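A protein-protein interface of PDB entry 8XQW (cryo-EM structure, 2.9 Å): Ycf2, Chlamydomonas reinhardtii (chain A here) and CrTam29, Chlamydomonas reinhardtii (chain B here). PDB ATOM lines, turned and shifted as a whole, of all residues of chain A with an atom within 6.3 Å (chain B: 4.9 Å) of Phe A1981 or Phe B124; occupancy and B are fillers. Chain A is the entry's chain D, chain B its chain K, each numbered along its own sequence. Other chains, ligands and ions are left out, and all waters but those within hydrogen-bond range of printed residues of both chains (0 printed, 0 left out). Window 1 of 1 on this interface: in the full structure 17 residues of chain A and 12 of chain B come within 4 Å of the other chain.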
ATOM      1  N   LYS A1979       5.047 -13.731 -17.245  1.00  0.00           N
ATOM      2  CA  LYS A1979       5.190 -12.570 -18.102  1.00  0.00           C
ATOM      3  C   LYS A1979       4.864 -11.309 -17.322  1.00  0.00           C
ATOM      4  O   LYS A1979       4.145 -11.340 -16.327  1.00  0.00           O
ATOM      5  CB  LYS A1979       4.279 -12.657 -19.319  1.00  0.00           C
ATOM      6  CG  LYS A1979       4.207 -14.014 -19.914  1.00  0.00           C
ATOM      7  CD  LYS A1979       4.720 -14.007 -21.314  1.00  0.00           C
ATOM      8  CE  LYS A1979       4.468 -15.340 -21.972  1.00  0.00           C
ATOM      9  NZ  LYS A1979       4.930 -15.346 -23.384  1.00  0.00           N
ATOM     10  N   THR A1980       5.396 -10.195 -17.797  1.00  0.00           N
ATOM     11  CA  THR A1980       5.175  -8.917 -17.153  1.00  0.00           C
ATOM     12  C   THR A1980       5.071  -7.853 -18.233  1.00  0.00           C
ATOM     13  O   THR A1980       5.246  -8.129 -19.417  1.00  0.00           O
ATOM     14  CB  THR A1980       6.291  -8.612 -16.157  1.00  0.00           C
ATOM     15  OG1 THR A1980       6.152  -7.273 -15.684  1.00  0.00           O
ATOM     16  CG2 THR A1980       7.644  -8.770 -16.804  1.00  0.00           C
ATOM     17  N   PHE A1981       4.785  -6.627 -17.819  1.00  0.00           N
ATOM     18  CA  PHE A1981       4.624  -5.553 -18.786  1.00  0.00           C
ATOM     19  C   PHE A1981       5.925  -5.139 -19.429  1.00  0.00           C
ATOM     20  O   PHE A1981       5.914  -4.270 -20.298  1.00  0.00           O
ATOM     21  CB  PHE A1981       3.977  -4.347 -18.124  1.00  0.00           C
ATOM     22  CG  PHE A1981       2.507  -4.473 -17.977  1.00  0.00           C
ATOM     23  CD1 PHE A1981       1.734  -4.883 -19.029  1.00  0.00           C
ATOM     24  CD2 PHE A1981       1.897  -4.200 -16.780  1.00  0.00           C
ATOM     25  CE1 PHE A1981       0.387  -5.005 -18.894  1.00  0.00           C
ATOM     26  CE2 PHE A1981       0.549  -4.326 -16.643  1.00  0.00           C
ATOM     27  CZ  PHE A1981      -0.205  -4.728 -17.703  1.00  0.00           C
ATOM     28  N   SER A1982       7.043  -5.725 -19.033  1.00  0.00           N
ATOM     29  CA  SER A1982       8.304  -5.430 -19.684  1.00  0.00           C
ATOM     30  C   SER A1982       8.602  -6.369 -20.836  1.00  0.00           C
ATOM     31  O   SER A1982       9.689  -6.286 -21.411  1.00  0.00           O
ATOM     32  CB  SER A1982       9.432  -5.480 -18.668  1.00  0.00           C
ATOM     33  OG  SER A1982       9.153  -4.618 -17.587  1.00  0.00           O
ATOM     34  N   HIS A1983       7.686  -7.273 -21.169  1.00  0.00           N
ATOM     35  CA  HIS A1983       7.777  -8.044 -22.396  1.00  0.00           C
ATOM     36  C   HIS A1983       7.116  -7.342 -23.567  1.00  0.00           C
ATOM     37  O   HIS A1983       7.203  -7.833 -24.692  1.00  0.00           O
ATOM     38  CB  HIS A1983       7.125  -9.408 -22.226  1.00  0.00           C
ATOM     39  CG  HIS A1983       7.826 -10.305 -21.261  1.00  0.00           C
ATOM     40  ND1 HIS A1983       8.534  -9.831 -20.180  1.00  0.00           N
ATOM     41  CD2 HIS A1983       7.917 -11.652 -21.208  1.00  0.00           C
ATOM     42  CE1 HIS A1983       9.028 -10.849 -19.501  1.00  0.00           C
ATOM     43  NE2 HIS A1983       8.668 -11.966 -20.105  1.00  0.00           N
ATOM     44  N   ILE A1984       6.445  -6.222 -23.324  1.00  0.00           N
ATOM     45  CA  ILE A1984       5.782  -5.446 -24.363  1.00  0.00           C
ATOM     46  C   ILE A1984       6.117  -3.980 -24.148  1.00  0.00           C
ATOM     47  O   ILE A1984       5.312  -3.249 -23.565  1.00  0.00           O
ATOM     48  CB  ILE A1984       4.263  -5.645 -24.336  1.00  0.00           C
ATOM     49  CG1 ILE A1984       3.858  -6.420 -23.098  1.00  0.00           C
ATOM     50  CG2 ILE A1984       3.794  -6.346 -25.586  1.00  0.00           C
ATOM     51  CD1 ILE A1984       2.489  -6.104 -22.646  1.00  0.00           C
ATOM     52  N   PRO A1985       7.280  -3.507 -24.582  1.00  0.00           N
ATOM     53  CA  PRO A1985       7.538  -2.066 -24.526  1.00  0.00           C
ATOM     54  C   PRO A1985       6.590  -1.256 -25.381  1.00  0.00           C
ATOM     55  O   PRO A1985       6.450  -0.053 -25.149  1.00  0.00           O
ATOM     56  CB  PRO A1985       8.978  -1.954 -25.027  1.00  0.00           C
ATOM     57  CG  PRO A1985       9.560  -3.267 -24.753  1.00  0.00           C
ATOM     58  CD  PRO A1985       8.479  -4.255 -24.969  1.00  0.00           C
ATOM     59  N   LEU A1987       3.541  -1.118 -25.280  1.00  0.00           N
ATOM     60  CA  LEU A1987       2.463  -0.575 -24.469  1.00  0.00           C
ATOM     61  C   LEU A1987       2.842   0.771 -23.877  1.00  0.00           C
ATOM     62  O   LEU A1987       1.969   1.566 -23.526  1.00  0.00           O
ATOM     63  CB  LEU A1987       2.102  -1.567 -23.365  1.00  0.00           C
ATOM     64  CG  LEU A1987       1.252  -1.100 -22.191  1.00  0.00           C
ATOM     65  CD1 LEU A1987      -0.166  -0.857 -22.629  1.00  0.00           C
ATOM     66  CD2 LEU A1987       1.284  -2.121 -21.098  1.00  0.00           C
ATOM     67  N   LEU A1993      -4.211   2.679 -24.672  1.00  0.00           N
ATOM     68  CA  LEU A1993      -4.272   1.472 -23.868  1.00  0.00           C
ATOM     69  C   LEU A1993      -4.081   1.728 -22.390  1.00  0.00           C
ATOM     70  O   LEU A1993      -4.231   0.798 -21.599  1.00  0.00           O
ATOM     71  CB  LEU A1993      -3.200   0.477 -24.312  1.00  0.00           C
ATOM     72  CG  LEU A1993      -3.648  -0.647 -25.223  1.00  0.00           C
ATOM     73  CD1 LEU A1993      -4.191  -0.047 -26.471  1.00  0.00           C
ATOM     74  CD2 LEU A1993      -2.473  -1.520 -25.538  1.00  0.00           C
ATOM     75  N   GLN A1994      -3.738   2.950 -22.002  1.00  0.00           N
ATOM     76  CA  GLN A1994      -3.343   3.192 -20.625  1.00  0.00           C
ATOM     77  C   GLN A1994      -4.532   3.113 -19.687  1.00  0.00           C
ATOM     78  O   GLN A1994      -4.433   2.539 -18.601  1.00  0.00           O
ATOM     79  CB  GLN A1994      -2.649   4.544 -20.506  1.00  0.00           C
ATOM     80  CG  GLN A1994      -1.612   4.811 -21.565  1.00  0.00           C
ATOM     81  CD  GLN A1994      -0.336   4.045 -21.359  1.00  0.00           C
ATOM     82  OE1 GLN A1994       0.541   4.050 -22.206  1.00  0.00           O
ATOM     83  NE2 GLN A1994      -0.216   3.391 -20.231  1.00  0.00           N
ATOM     84  N   GLN A1995      -5.673   3.662 -20.084  1.00  0.00           N
ATOM     85  CA  GLN A1995      -6.776   3.734 -19.131  1.00  0.00           C
ATOM     86  C   GLN A1995      -7.465   2.397 -18.915  1.00  0.00           C
ATOM     87  O   GLN A1995      -7.658   2.018 -17.749  1.00  0.00           O
ATOM     88  CB  GLN A1995      -7.768   4.813 -19.547  1.00  0.00           C
ATOM     89  CG  GLN A1995      -9.003   4.781 -18.707  1.00  0.00           C
ATOM     90  CD  GLN A1995      -9.917   5.915 -19.013  1.00  0.00           C
ATOM     91  OE1 GLN A1995      -9.623   6.734 -19.874  1.00  0.00           O
ATOM     92  NE2 GLN A1995     -11.035   5.983 -18.316  1.00  0.00           N
ATOM     93  N   ILE A1997      -6.374  -0.801 -19.372  1.00  0.00           N
ATOM     94  CA  ILE A1997      -5.455  -1.715 -18.710  1.00  0.00           C
ATOM     95  C   ILE A1997      -5.117  -1.225 -17.310  1.00  0.00           C
ATOM     96  O   ILE A1997      -5.058  -2.015 -16.361  1.00  0.00           O
ATOM     97  CB  ILE A1997      -4.199  -1.904 -19.569  1.00  0.00           C
ATOM     98  CG1 ILE A1997      -4.591  -2.374 -20.959  1.00  0.00           C
ATOM     99  CG2 ILE A1997      -3.302  -2.927 -18.965  1.00  0.00           C
ATOM    100  CD1 ILE A1997      -5.318  -3.682 -20.958  1.00  0.00           C
ATOM    101  N   GLY A1998      -4.901   0.080 -17.148  1.00  0.00           N
ATOM    102  CA  GLY A1998      -4.583   0.601 -15.834  1.00  0.00           C
ATOM    103  C   GLY A1998      -5.715   0.441 -14.849  1.00  0.00           C
ATOM    104  O   GLY A1998      -5.484   0.107 -13.684  1.00  0.00           O
ATOM    105  N   SER A1999      -6.947   0.661 -15.294  1.00  0.00           N
ATOM    106  CA  SER A1999      -8.085   0.445 -14.421  1.00  0.00           C
ATOM    107  C   SER A1999      -8.180  -1.009 -14.003  1.00  0.00           C
ATOM    108  O   SER A1999      -8.402  -1.309 -12.826  1.00  0.00           O
ATOM    109  CB  SER A1999      -9.361   0.880 -15.124  1.00  0.00           C
ATOM    110  OG  SER A1999      -9.521   2.278 -15.045  1.00  0.00           O
ATOM    111  N   VAL A2001      -5.794  -3.168 -13.709  1.00  0.00           N
ATOM    112  CA  VAL A2001      -4.728  -3.523 -12.778  1.00  0.00           C
ATOM    113  C   VAL A2001      -5.016  -2.960 -11.396  1.00  0.00           C
ATOM    114  O   VAL A2001      -4.872  -3.656 -10.385  1.00  0.00           O
ATOM    115  CB  VAL A2001      -3.368  -3.050 -13.311  1.00  0.00           C
ATOM    116  CG1 VAL A2001      -2.320  -3.257 -12.271  1.00  0.00           C
ATOM    117  CG2 VAL A2001      -3.012  -3.814 -14.534  1.00  0.00           C
ATOM    118  N   LEU A2036      -0.256  -9.377 -24.756  1.00  0.00           N
ATOM    119  CA  LEU A2036      -0.672  -8.317 -23.849  1.00  0.00           C
ATOM    120  C   LEU A2036      -1.560  -8.858 -22.742  1.00  0.00           C
ATOM    121  O   LEU A2036      -1.439  -8.450 -21.582  1.00  0.00           O
ATOM    122  CB  LEU A2036      -1.390  -7.223 -24.623  1.00  0.00           C
ATOM    123  CG  LEU A2036      -1.971  -6.098 -23.782  1.00  0.00           C
ATOM    124  CD1 LEU A2036      -0.938  -5.037 -23.582  1.00  0.00           C
ATOM    125  CD2 LEU A2036      -3.180  -5.520 -24.455  1.00  0.00           C
ATOM    126  N   ALA A2039       0.549 -10.780 -20.283  1.00  0.00           N
ATOM    127  CA  ALA A2039       1.281  -9.848 -19.439  1.00  0.00           C
ATOM    128  C   ALA A2039       0.388  -9.259 -18.361  1.00  0.00           C
ATOM    129  O   ALA A2039       0.827  -9.081 -17.224  1.00  0.00           O
ATOM    130  CB  ALA A2039       1.887  -8.738 -20.285  1.00  0.00           C
ATOM    131  N   LEU A2040      -0.857  -8.944 -18.697  1.00  0.00           N
ATOM    132  CA  LEU A2040      -1.782  -8.470 -17.675  1.00  0.00           C
ATOM    133  C   LEU A2040      -2.051  -9.538 -16.625  1.00  0.00           C
ATOM    134  O   LEU A2040      -2.198  -9.228 -15.441  1.00  0.00           O
ATOM    135  CB  LEU A2040      -3.085  -8.019 -18.318  1.00  0.00           C
ATOM    136  CG  LEU A2040      -4.274  -7.845 -17.387  1.00  0.00           C
ATOM    137  CD1 LEU A2040      -4.098  -6.612 -16.577  1.00  0.00           C
ATOM    138  CD2 LEU A2040      -5.531  -7.764 -18.181  1.00  0.00           C
ATOM    139  N   GLU A2043       1.436  -9.950 -14.525  1.00  0.00           N
ATOM    140  CA  GLU A2043       1.799  -8.834 -13.667  1.00  0.00           C
ATOM    141  C   GLU A2043       1.020  -8.855 -12.365  1.00  0.00           C
ATOM    142  O   GLU A2043       1.559  -8.503 -11.316  1.00  0.00           O
ATOM    143  CB  GLU A2043       1.564  -7.519 -14.399  1.00  0.00           C
ATOM    144  CG  GLU A2043       2.106  -6.308 -13.685  1.00  0.00           C
ATOM    145  CD  GLU A2043       3.505  -5.951 -14.135  1.00  0.00           C
ATOM    146  OE1 GLU A2043       4.026  -4.897 -13.719  1.00  0.00           O
ATOM    147  OE2 GLU A2043       4.091  -6.726 -14.904  1.00  0.00           O
ATOM    148  N   TRP B 120      -2.465   7.723 -16.152  1.00  0.00           N
ATOM    149  CA  TRP B 120      -2.227   6.293 -16.067  1.00  0.00           C
ATOM    150  C   TRP B 120      -0.867   5.918 -16.617  1.00  0.00           C
ATOM    151  O   TRP B 120      -0.276   4.930 -16.183  1.00  0.00           O
ATOM    152  CB  TRP B 120      -3.322   5.546 -16.798  1.00  0.00           C
ATOM    153  CG  TRP B 120      -4.622   5.666 -16.134  1.00  0.00           C
ATOM    154  CD1 TRP B 120      -5.120   4.855 -15.170  1.00  0.00           C
ATOM    155  CD2 TRP B 120      -5.601   6.671 -16.362  1.00  0.00           C
ATOM    156  NE1 TRP B 120      -6.354   5.288 -14.781  1.00  0.00           N
ATOM    157  CE2 TRP B 120      -6.674   6.405 -15.503  1.00  0.00           C
ATOM    158  CE3 TRP B 120      -5.678   7.775 -17.210  1.00  0.00           C
ATOM    159  CZ2 TRP B 120      -7.811   7.200 -15.469  1.00  0.00           C
ATOM    160  CZ3 TRP B 120      -6.807   8.565 -17.173  1.00  0.00           C
ATOM    161  CH2 TRP B 120      -7.858   8.274 -16.312  1.00  0.00           C
ATOM    162  N   GLN B 121      -0.348   6.688 -17.560  1.00  0.00           N
ATOM    163  CA  GLN B 121       0.991   6.406 -18.042  1.00  0.00           C
ATOM    164  C   GLN B 121       2.014   6.613 -16.949  1.00  0.00           C
ATOM    165  O   GLN B 121       2.953   5.828 -16.808  1.00  0.00           O
ATOM    166  CB  GLN B 121       1.323   7.285 -19.229  1.00  0.00           C
ATOM    167  CG  GLN B 121       2.773   7.251 -19.568  1.00  0.00           C
ATOM    168  CD  GLN B 121       3.061   7.907 -20.866  1.00  0.00           C
ATOM    169  OE1 GLN B 121       3.037   7.268 -21.908  1.00  0.00           O
ATOM    170  NE2 GLN B 121       3.344   9.194 -20.825  1.00  0.00           N
ATOM    171  N   ASP B 122       1.851   7.667 -16.161  1.00  0.00           N
ATOM    172  CA  ASP B 122       2.774   7.898 -15.065  1.00  0.00           C
ATOM    173  C   ASP B 122       2.682   6.791 -14.034  1.00  0.00           C
ATOM    174  O   ASP B 122       3.697   6.364 -13.476  1.00  0.00           O
ATOM    175  CB  ASP B 122       2.488   9.241 -14.430  1.00  0.00           C
ATOM    176  CG  ASP B 122       3.377   9.517 -13.273  1.00  0.00           C
ATOM    177  OD1 ASP B 122       4.590   9.703 -13.495  1.00  0.00           O
ATOM    178  OD2 ASP B 122       2.866   9.544 -12.137  1.00  0.00           O
ATOM    179  N   LYS B 123       1.472   6.317 -13.758  1.00  0.00           N
ATOM    180  CA  LYS B 123       1.347   5.178 -12.854  1.00  0.00           C
ATOM    181  C   LYS B 123       2.106   3.971 -13.379  1.00  0.00           C
ATOM    182  O   LYS B 123       2.869   3.343 -12.647  1.00  0.00           O
ATOM    183  CB  LYS B 123      -0.111   4.825 -12.640  1.00  0.00           C
ATOM    184  CG  LYS B 123      -0.717   5.573 -11.519  1.00  0.00           C
ATOM    185  CD  LYS B 123      -2.149   5.243 -11.406  1.00  0.00           C
ATOM    186  CE  LYS B 123      -2.897   6.422 -10.909  1.00  0.00           C
ATOM    187  NZ  LYS B 123      -4.298   6.317 -11.335  1.00  0.00           N
ATOM    188  N   PHE B 124       1.905   3.626 -14.648  1.00  0.00           N
ATOM    189  CA  PHE B 124       2.640   2.509 -15.239  1.00  0.00           C
ATOM    190  C   PHE B 124       4.142   2.701 -15.123  1.00  0.00           C
ATOM    191  O   PHE B 124       4.878   1.743 -14.878  1.00  0.00           O
ATOM    192  CB  PHE B 124       2.269   2.353 -16.706  1.00  0.00           C
ATOM    193  CG  PHE B 124       1.138   1.434 -16.943  1.00  0.00           C
ATOM    194  CD1 PHE B 124      -0.153   1.869 -16.818  1.00  0.00           C
ATOM    195  CD2 PHE B 124       1.363   0.136 -17.299  1.00  0.00           C
ATOM    196  CE1 PHE B 124      -1.187   1.026 -17.040  1.00  0.00           C
ATOM    197  CE2 PHE B 124       0.325  -0.706 -17.518  1.00  0.00           C
ATOM    198  CZ  PHE B 124      -0.948  -0.263 -17.388  1.00  0.00           C
ATOM    199  N   MET B 125       4.621   3.924 -15.320  1.00  0.00           N
ATOM    200  CA  MET B 125       6.060   4.154 -15.339  1.00  0.00           C
ATOM    201  C   MET B 125       6.663   4.012 -13.952  1.00  0.00           C
ATOM    202  O   MET B 125       7.733   3.423 -13.789  1.00  0.00           O
ATOM    203  CB  MET B 125       6.364   5.531 -15.911  1.00  0.00           C
ATOM    204  CG  MET B 125       6.319   5.585 -17.407  1.00  0.00           C
ATOM    205  SD  MET B 125       7.364   6.873 -18.092  1.00  0.00           S
ATOM    206  CE  MET B 125       6.602   8.323 -17.388  1.00  0.00           C
ATOM    207  N   ARG B 126       6.004   4.562 -12.939  1.00  0.00           N
ATOM    208  CA  ARG B 126       6.557   4.468 -11.594  1.00  0.00           C
ATOM    209  C   ARG B 126       6.390   3.082 -11.002  1.00  0.00           C
ATOM    210  O   ARG B 126       7.229   2.645 -10.214  1.00  0.00           O
ATOM    211  CB  ARG B 126       5.899   5.486 -10.688  1.00  0.00           C
ATOM    212  CG  ARG B 126       6.095   6.883 -11.145  1.00  0.00           C
ATOM    213  CD  ARG B 126       5.477   7.820 -10.173  1.00  0.00           C
ATOM    214  NE  ARG B 126       6.385   8.099  -9.077  1.00  0.00           N
ATOM    215  CZ  ARG B 126       6.199   7.672  -7.840  1.00  0.00           C
ATOM    216  NH1 ARG B 126       5.131   6.946  -7.550  1.00  0.00           N
ATOM    217  NH2 ARG B 126       7.074   7.975  -6.897  1.00  0.00           N
ATOM    218  N   CYS B 127       5.328   2.379 -11.358  1.00  0.00           N
ATOM    219  CA  CYS B 127       5.072   1.082 -10.758  1.00  0.00           C
ATOM    220  C   CYS B 127       5.710  -0.064 -11.520  1.00  0.00           C
ATOM    221  O   CYS B 127       6.042  -1.079 -10.914  1.00  0.00           O
ATOM    222  CB  CYS B 127       3.573   0.847 -10.645  1.00  0.00           C
ATOM    223  SG  CYS B 127       2.701   2.130  -9.751  1.00  0.00           S
ATOM    224  N   SER B 128       5.875   0.039 -12.809  1.00  0.00           N
ATOM    225  CA  SER B 128       6.300  -1.211 -13.416  1.00  0.00           C
ATOM    226  C   SER B 128       7.512  -1.116 -14.330  1.00  0.00           C
ATOM    227  O   SER B 128       8.357  -2.005 -14.287  1.00  0.00           O
ATOM    228  CB  SER B 128       5.139  -1.814 -14.190  1.00  0.00           C
ATOM    229  OG  SER B 128       5.498  -3.079 -14.704  1.00  0.00           O
ATOM    230  N   THR B 129       7.631  -0.076 -15.151  1.00  0.00           N
ATOM    231  CA  THR B 129       8.533  -0.163 -16.294  1.00  0.00           C
ATOM    232  C   THR B 129       9.772   0.710 -16.205  1.00  0.00           C
ATOM    233  O   THR B 129      10.751   0.417 -16.892  1.00  0.00           O
ATOM    234  CB  THR B 129       7.793   0.171 -17.594  1.00  0.00           C
ATOM    235  OG1 THR B 129       7.471   1.560 -17.614  1.00  0.00           O
ATOM    236  CG2 THR B 129       6.523  -0.632 -17.714  1.00  0.00           C
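Printed residues of chain A that touch a printed residue of chain B: Phe A1981, Leu A1987, Gln A1994, Ile A1997, Gly A1998 and Glu A2043. Of the 10 printed residues of chain B, 4 touch a printed residue of chain A. Hydrophobic or aromatic side chains of chain B within 4 Å of the printed part of chain A: Trp B120 and Phe B124. Among the printed residues, no Asp or Glu carboxylate lies within 4 Å of a Lys or Arg side-chain nitrogen of the other chain.
Among the printed residues, merely in contact across the chains: Gly A1998 with Phe B124 (3.6 Å), Gln A1994 with Trp B120 (3.7 Å), Phe A1981 with Phe B124 (3.7 Å), Gln A1994 with Phe B124 (3.7 Å), Ile A1997 with Phe B124 (3.9 Å), Gln A1994 with Gln B121 (3.9 Å), Phe A1981 with Ser B128 (3.95 Å) and Leu A1987 with Phe B124 (3.97 Å).
OE1 of Glu A2043 lies within hydrogen-bond range of OG of Ser B128 (2.5 Å).
The backbone carbonyl oxygen of Phe B124 is in hydrogen-bond range of the backbone NH of Thr B129 (3.3 Å). The side-chain carboxylate (OE2) of Glu A2043 lies within hydrogen-bond range of the backbone NH (N) of Phe A1981. The backbone carbonyl oxygen (O) of Leu A1987 sits close to the side-chain amide oxygen (OE1) of Gln A1994, at 3.2 Å.
Phe A1981 touches just these residues of chain B: Phe B124 (3.7 Å) and Ser B128 (3.95 Å). His A1983 touches none of the printed residues of chain B. Of the printed residues of chain B, Leu A1987 touches Phe B124. Printed residues of chain B within 4 Å of Glu A2043: Ser B128. Of chain A, only Phe A1981 (3.7 Å), Leu A1987 (3.97 Å), Gln A1994 (3.7 Å), Ile A1997 (3.9 Å) and Gly A1998 (3.6 Å) come within 4 Å of Phe B124. Cys B127 touches none of the printed residues of chain A. The nearest residue of chain A that does not touch Phe B124 is Val A2001 (5.0 Å).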
